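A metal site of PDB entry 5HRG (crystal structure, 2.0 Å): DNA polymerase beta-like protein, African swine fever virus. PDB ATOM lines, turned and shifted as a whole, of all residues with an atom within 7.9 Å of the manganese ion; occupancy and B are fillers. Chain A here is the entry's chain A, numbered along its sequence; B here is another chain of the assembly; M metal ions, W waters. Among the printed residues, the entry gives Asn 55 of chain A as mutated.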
ATOM      1  N   VAL A  41       8.459 -17.820 -12.468  1.00  0.00           N
ATOM      2  CA  VAL A  41       8.229 -18.271 -13.830  1.00  0.00           C
ATOM      3  C   VAL A  41       9.409 -19.141 -14.281  1.00  0.00           C
ATOM      4  O   VAL A  41      10.203 -19.564 -13.447  1.00  0.00           O
ATOM      5  CB  VAL A  41       7.986 -17.076 -14.787  1.00  0.00           C
ATOM      6  CG1 VAL A  41       6.631 -16.445 -14.467  1.00  0.00           C
ATOM      7  CG2 VAL A  41       9.101 -16.046 -14.681  1.00  0.00           C
ATOM      8  N   GLY A  42       9.500 -19.433 -15.572  1.00  0.00           N
ATOM      9  CA  GLY A  42      10.610 -20.200 -16.104  1.00  0.00           C
ATOM     10  C   GLY A  42      10.565 -21.649 -15.649  1.00  0.00           C
ATOM     11  O   GLY A  42       9.497 -22.197 -15.359  1.00  0.00           O
ATOM     12  N   SER A  43      11.739 -22.255 -15.579  1.00  0.00           N
ATOM     13  CA  SER A  43      11.850 -23.691 -15.298  1.00  0.00           C
ATOM     14  C   SER A  43      11.310 -24.089 -13.913  1.00  0.00           C
ATOM     15  O   SER A  43      10.813 -25.201 -13.723  1.00  0.00           O
ATOM     16  CB  SER A  43      13.301 -24.149 -15.456  1.00  0.00           C
ATOM     17  OG  SER A  43      14.176 -23.353 -14.661  1.00  0.00           O
ATOM     18  N   ASN A  52      18.902 -23.690 -13.955  1.00  0.00           N
ATOM     19  CA  ASN A  52      20.110 -22.932 -14.242  1.00  0.00           C
ATOM     20  C   ASN A  52      20.081 -21.551 -13.587  1.00  0.00           C
ATOM     21  O   ASN A  52      21.124 -20.927 -13.424  1.00  0.00           O
ATOM     22  CB  ASN A  52      20.281 -22.756 -15.737  1.00  0.00           C
ATOM     23  CG  ASN A  52      20.341 -24.083 -16.472  1.00  0.00           C
ATOM     24  OD1 ASN A  52      21.097 -24.966 -16.096  1.00  0.00           O
ATOM     25  ND2 ASN A  52      19.529 -24.225 -17.520  1.00  0.00           N
ATOM     26  N   ASP A  53      18.886 -21.080 -13.255  1.00  0.00           N
ATOM     27  CA  ASP A  53      18.738 -19.795 -12.560  1.00  0.00           C
ATOM     28  C   ASP A  53      17.348 -19.661 -11.949  1.00  0.00           C
ATOM     29  O   ASP A  53      16.547 -20.608 -11.990  1.00  0.00           O
ATOM     30  CB  ASP A  53      19.037 -18.623 -13.527  1.00  0.00           C
ATOM     31  CG  ASP A  53      17.942 -18.373 -14.533  1.00  0.00           C
ATOM     32  OD1 ASP A  53      17.150 -19.276 -14.853  1.00  0.00           O
ATOM     33  OD2 ASP A  53      17.876 -17.231 -15.034  1.00  0.00           O
ATOM     34  N   VAL A  54      17.076 -18.492 -11.359  1.00  0.00           N
ATOM     35  CA  VAL A  54      15.761 -18.170 -10.806  1.00  0.00           C
ATOM     36  C   VAL A  54      15.170 -17.006 -11.610  1.00  0.00           C
ATOM     37  O   VAL A  54      15.873 -16.066 -11.971  1.00  0.00           O
ATOM     38  CB  VAL A  54      15.853 -17.762  -9.319  1.00  0.00           C
ATOM     39  CG1 VAL A  54      14.473 -17.473  -8.756  1.00  0.00           C
ATOM     40  CG2 VAL A  54      16.528 -18.861  -8.509  1.00  0.00           C
ATOM     41  N   ASN A  55      13.873 -17.102 -11.901  1.00  0.00           N
ATOM     42  CA  ASN A  55      13.161 -16.148 -12.724  1.00  0.00           C
ATOM     43  C   ASN A  55      11.895 -15.668 -12.033  1.00  0.00           C
ATOM     44  O   ASN A  55      11.040 -16.488 -11.664  1.00  0.00           O
ATOM     45  CB  ASN A  55      12.800 -16.764 -14.070  1.00  0.00           C
ATOM     46  CG  ASN A  55      14.017 -17.345 -14.785  1.00  0.00           C
ATOM     47  OD1 ASN A  55      14.790 -16.638 -15.426  1.00  0.00           O
ATOM     48  ND2 ASN A  55      14.209 -18.650 -14.640  1.00  0.00           N
ATOM     49  N   LEU A  56      11.779 -14.349 -11.844  1.00  0.00           N
ATOM     50  CA  LEU A  56      10.582 -13.766 -11.249  1.00  0.00           C
ATOM     51  C   LEU A  56       9.930 -12.767 -12.193  1.00  0.00           C
ATOM     52  O   LEU A  56      10.604 -11.922 -12.790  1.00  0.00           O
ATOM     53  CB  LEU A  56      10.908 -13.072  -9.925  1.00  0.00           C
ATOM     54  CG  LEU A  56      11.442 -13.920  -8.767  1.00  0.00           C
ATOM     55  CD1 LEU A  56      11.715 -13.042  -7.561  1.00  0.00           C
ATOM     56  CD2 LEU A  56      10.471 -15.034  -8.405  1.00  0.00           C
ATOM     57  N   LYS A  89      13.487  -6.125 -18.403  1.00  0.00           N
ATOM     58  CA  LYS A  89      14.323  -7.263 -18.043  1.00  0.00           C
ATOM     59  C   LYS A  89      15.538  -6.772 -17.267  1.00  0.00           C
ATOM     60  O   LYS A  89      16.222  -5.845 -17.688  1.00  0.00           O
ATOM     61  CB  LYS A  89      14.772  -8.035 -19.275  1.00  0.00           C
ATOM     62  CG  LYS A  89      15.698  -9.225 -19.008  1.00  0.00           C
ATOM     63  CD  LYS A  89      16.567  -9.519 -20.237  1.00  0.00           C
ATOM     64  CE  LYS A  89      17.505 -10.707 -20.023  1.00  0.00           C
ATOM     65  N   VAL A  91      18.863  -8.609 -15.109  1.00  0.00           N
ATOM     66  CA  VAL A  91      19.610  -9.790 -14.685  1.00  0.00           C
ATOM     67  C   VAL A  91      20.468  -9.425 -13.469  1.00  0.00           C
ATOM     68  O   VAL A  91      21.265  -8.496 -13.525  1.00  0.00           O
ATOM     69  CB  VAL A  91      20.527 -10.321 -15.800  1.00  0.00           C
ATOM     70  CG1 VAL A  91      21.251 -11.585 -15.351  1.00  0.00           C
ATOM     71  CG2 VAL A  91      19.747 -10.587 -17.083  1.00  0.00           C
ATOM     72  N   GLN A 102      22.113 -16.748 -10.735  1.00  0.00           N
ATOM     73  CA  GLN A 102      21.487 -15.782 -11.621  1.00  0.00           C
ATOM     74  C   GLN A 102      20.027 -15.622 -11.242  1.00  0.00           C
ATOM     75  O   GLN A 102      19.302 -16.608 -11.020  1.00  0.00           O
ATOM     76  CB  GLN A 102      21.628 -16.209 -13.067  1.00  0.00           C
ATOM     77  CG  GLN A 102      20.929 -15.274 -14.049  1.00  0.00           C
ATOM     78  CD  GLN A 102      21.373 -15.520 -15.474  1.00  0.00           C
ATOM     79  OE1 GLN A 102      22.531 -15.837 -15.722  1.00  0.00           O
ATOM     80  NE2 GLN A 102      20.462 -15.335 -16.418  1.00  0.00           N
ATOM     81  N   LEU A 103      19.596 -14.371 -11.137  1.00  0.00           N
ATOM     82  CA  LEU A 103      18.220 -14.056 -10.846  1.00  0.00           C
ATOM     83  C   LEU A 103      17.726 -13.125 -11.942  1.00  0.00           C
ATOM     84  O   LEU A 103      18.190 -11.993 -12.026  1.00  0.00           O
ATOM     85  CB  LEU A 103      18.109 -13.386  -9.463  1.00  0.00           C
ATOM     86  CG  LEU A 103      16.740 -12.776  -9.118  1.00  0.00           C
ATOM     87  CD1 LEU A 103      15.683 -13.873  -9.105  1.00  0.00           C
ATOM     88  CD2 LEU A 103      16.772 -12.058  -7.768  1.00  0.00           C
ATOM     89  N   ASP A 104      16.814 -13.608 -12.775  1.00  0.00           N
ATOM     90  CA  ASP A 104      16.232 -12.806 -13.841  1.00  0.00           C
ATOM     91  C   ASP A 104      14.918 -12.198 -13.347  1.00  0.00           C
ATOM     92  O   ASP A 104      14.066 -12.913 -12.802  1.00  0.00           O
ATOM     93  CB  ASP A 104      15.951 -13.641 -15.090  1.00  0.00           C
ATOM     94  CG  ASP A 104      17.217 -14.033 -15.852  1.00  0.00           C
ATOM     95  OD1 ASP A 104      18.290 -13.423 -15.637  1.00  0.00           O
ATOM     96  OD2 ASP A 104      17.130 -14.968 -16.676  1.00  0.00           O
ATOM     97  N   LEU A 105      14.778 -10.891 -13.507  1.00  0.00           N
ATOM     98  CA  LEU A 105      13.549 -10.198 -13.152  1.00  0.00           C
ATOM     99  C   LEU A 105      12.917  -9.654 -14.408  1.00  0.00           C
ATOM    100  O   LEU A 105      13.614  -9.089 -15.273  1.00  0.00           O
ATOM    101  CB  LEU A 105      13.815  -9.060 -12.169  1.00  0.00           C
ATOM    102  CG  LEU A 105      14.531  -9.431 -10.870  1.00  0.00           C
ATOM    103  CD1 LEU A 105      14.678  -8.189 -10.010  1.00  0.00           C
ATOM    104  CD2 LEU A 105      13.771 -10.515 -10.106  1.00  0.00           C
ATOM    105  N   PHE A 106      11.605  -9.837 -14.497  1.00  0.00           N
ATOM    106  CA  PHE A 106      10.841  -9.312 -15.614  1.00  0.00           C
ATOM    107  C   PHE A 106       9.642  -8.552 -15.079  1.00  0.00           C
ATOM    108  O   PHE A 106       9.166  -8.837 -13.978  1.00  0.00           O
ATOM    109  CB  PHE A 106      10.362 -10.438 -16.535  1.00  0.00           C
ATOM    110  CG  PHE A 106      11.442 -11.407 -16.940  1.00  0.00           C
ATOM    111  CD1 PHE A 106      12.257 -11.152 -18.045  1.00  0.00           C
ATOM    112  CD2 PHE A 106      11.627 -12.578 -16.244  1.00  0.00           C
ATOM    113  CE1 PHE A 106      13.236 -12.053 -18.425  1.00  0.00           C
ATOM    114  CE2 PHE A 106      12.612 -13.489 -16.616  1.00  0.00           C
ATOM    115  CZ  PHE A 106      13.414 -13.217 -17.712  1.00  0.00           C
ATOM    116  P    DC B   6      24.846 -15.436 -24.963  1.00  0.00           P
ATOM    117  OP1  DC B   6      25.858 -15.624 -23.899  1.00  0.00           O
ATOM    118  OP2  DC B   6      24.663 -16.489 -25.982  1.00  0.00           O
ATOM    119  O5'  DC B   6      23.422 -15.132 -24.319  1.00  0.00           O
ATOM    120  C5'  DC B   6      23.290 -14.225 -23.213  1.00  0.00           C
ATOM    121  C4'  DC B   6      21.888 -13.687 -23.137  1.00  0.00           C
ATOM    122  O4'  DC B   6      21.468 -13.210 -24.422  1.00  0.00           O
ATOM    123  C3'  DC B   6      20.823 -14.705 -22.758  1.00  0.00           C
ATOM    124  O3'  DC B   6      20.657 -14.899 -21.356  1.00  0.00           O
ATOM    125  C2'  DC B   6      19.557 -14.078 -23.308  1.00  0.00           C
ATOM    126  C1'  DC B   6      20.046 -13.124 -24.399  1.00  0.00           C
ATOM    127  N1   DC B   6      19.523 -13.443 -25.733  1.00  0.00           N
ATOM    128  C2   DC B   6      18.350 -12.799 -26.139  1.00  0.00           C
ATOM    129  O2   DC B   6      17.828 -11.972 -25.370  1.00  0.00           O
ATOM    130  N3   DC B   6      17.832 -13.082 -27.348  1.00  0.00           N
ATOM    131  C4   DC B   6      18.431 -13.980 -28.139  1.00  0.00           C
ATOM    132  N4   DC B   6      17.878 -14.227 -29.331  1.00  0.00           N
ATOM    133  C5   DC B   6      19.616 -14.664 -27.747  1.00  0.00           C
ATOM    134  C6   DC B   6      20.122 -14.376 -26.533  1.00  0.00           C
ATOM    135  P    DG B   7      19.825 -16.165 -20.833  1.00  0.00           P
ATOM    136  OP1  DG B   7      20.141 -16.352 -19.397  1.00  0.00           O
ATOM    137  OP2  DG B   7      20.014 -17.292 -21.794  1.00  0.00           O
ATOM    138  O5'  DG B   7      18.320 -15.683 -20.969  1.00  0.00           O
ATOM    139  C5'  DG B   7      17.823 -14.627 -20.134  1.00  0.00           C
ATOM    140  C4'  DG B   7      16.354 -14.400 -20.405  1.00  0.00           C
ATOM    141  O4'  DG B   7      16.178 -13.660 -21.633  1.00  0.00           O
ATOM    142  C3'  DG B   7      15.499 -15.647 -20.597  1.00  0.00           C
ATOM    143  O3'  DG B   7      15.169 -16.241 -19.349  1.00  0.00           O
ATOM    144  C2'  DG B   7      14.284 -15.069 -21.302  1.00  0.00           C
ATOM    145  C1'  DG B   7      14.926 -14.040 -22.215  1.00  0.00           C
ATOM    146  N9   DG B   7      15.196 -14.547 -23.556  1.00  0.00           N
ATOM    147  C8   DG B   7      16.309 -15.249 -23.975  1.00  0.00           C
ATOM    148  N7   DG B   7      16.260 -15.580 -25.236  1.00  0.00           N
ATOM    149  C5   DG B   7      15.047 -15.086 -25.677  1.00  0.00           C
ATOM    150  C6   DG B   7      14.442 -15.129 -26.959  1.00  0.00           C
ATOM    151  O6   DG B   7      14.883 -15.658 -27.996  1.00  0.00           O
ATOM    152  N1   DG B   7      13.202 -14.500 -26.972  1.00  0.00           N
ATOM    153  C2   DG B   7      12.626 -13.897 -25.881  1.00  0.00           C
ATOM    154  N2   DG B   7      11.418 -13.346 -26.090  1.00  0.00           N
ATOM    155  N3   DG B   7      13.172 -13.841 -24.684  1.00  0.00           N
ATOM    156  C4   DG B   7      14.371 -14.452 -24.648  1.00  0.00           C
ATOM    157  P    DC B   8      15.131 -17.844 -19.184  1.00  0.00           P
ATOM    158  OP1  DC B   8      15.385 -18.153 -17.745  1.00  0.00           O
ATOM    159  OP2  DC B   8      16.016 -18.417 -20.214  1.00  0.00           O
ATOM    160  O5'  DC B   8      13.644 -18.222 -19.583  1.00  0.00           O
ATOM    161  C5'  DC B   8      12.511 -17.629 -18.932  1.00  0.00           C
ATOM    162  C4'  DC B   8      11.317 -17.639 -19.849  1.00  0.00           C
ATOM    163  O4'  DC B   8      11.575 -16.790 -20.999  1.00  0.00           O
ATOM    164  C3'  DC B   8      10.942 -18.990 -20.456  1.00  0.00           C
ATOM    165  O3'  DC B   8      10.139 -19.780 -19.575  1.00  0.00           O
ATOM    166  C2'  DC B   8      10.162 -18.573 -21.695  1.00  0.00           C
ATOM    167  C1'  DC B   8      10.859 -17.287 -22.130  1.00  0.00           C
ATOM    168  N1   DC B   8      11.824 -17.490 -23.221  1.00  0.00           N
ATOM    169  C2   DC B   8      11.423 -17.188 -24.531  1.00  0.00           C
ATOM    170  O2   DC B   8      10.303 -16.707 -24.712  1.00  0.00           O
ATOM    171  N3   DC B   8      12.287 -17.407 -25.552  1.00  0.00           N
ATOM    172  C4   DC B   8      13.492 -17.924 -25.300  1.00  0.00           C
ATOM    173  N4   DC B   8      14.314 -18.127 -26.344  1.00  0.00           N
ATOM    174  C5   DC B   8      13.919 -18.252 -23.982  1.00  0.00           C
ATOM    175  C6   DC B   8      13.054 -18.029 -22.985  1.00  0.00           C
HETATM  176 MN    MN M   1      16.558 -16.937 -16.568  1.00  0.00          MN
HETATM  177  O   HOH W   1      18.241 -17.696 -18.063  1.00  0.00           O
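The side-chain carboxylate of Asp 53 sits close to the side-chain amide nitrogen of Gln 102.
The side-chain amide nitrogen (NE2) of Gln 102 is in hydrogen-bond range of the side-chain carboxylate (OD1) of Asp 104, 3.0 Å away.
N of Asp 104 is in hydrogen-bond range of O of Val 54, 2.8 Å away.
O of Asp 104 is in hydrogen-bond range of N of Leu 56, at 2.9 Å.
The backbone carbonyl oxygen (O) of Asn 55 lies within hydrogen-bond range of the backbone NH (N) of Val 41, 3.0 Å away.
The side-chain amide nitrogen (NE2) of Gln 102 lies within hydrogen-bond range of OP1 of DG 7 of chain B (3.2 Å).
Residues that only touch the manganese ion: DG 7 of chain B.
The manganese ion is bound by the side-chain carboxylate (OD2) of Asp 53 (2.0 Å), the side-chain carboxylate (OD2) of Asp 104 (2.1 Å), OP1 of DC 8 of chain B (2.1 Å), the side-chain amide oxygen (OD1) of Asn 55 (2.1 Å) and water W1 (2.4 Å).
The manganese ion has five donor atoms within binding distance.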
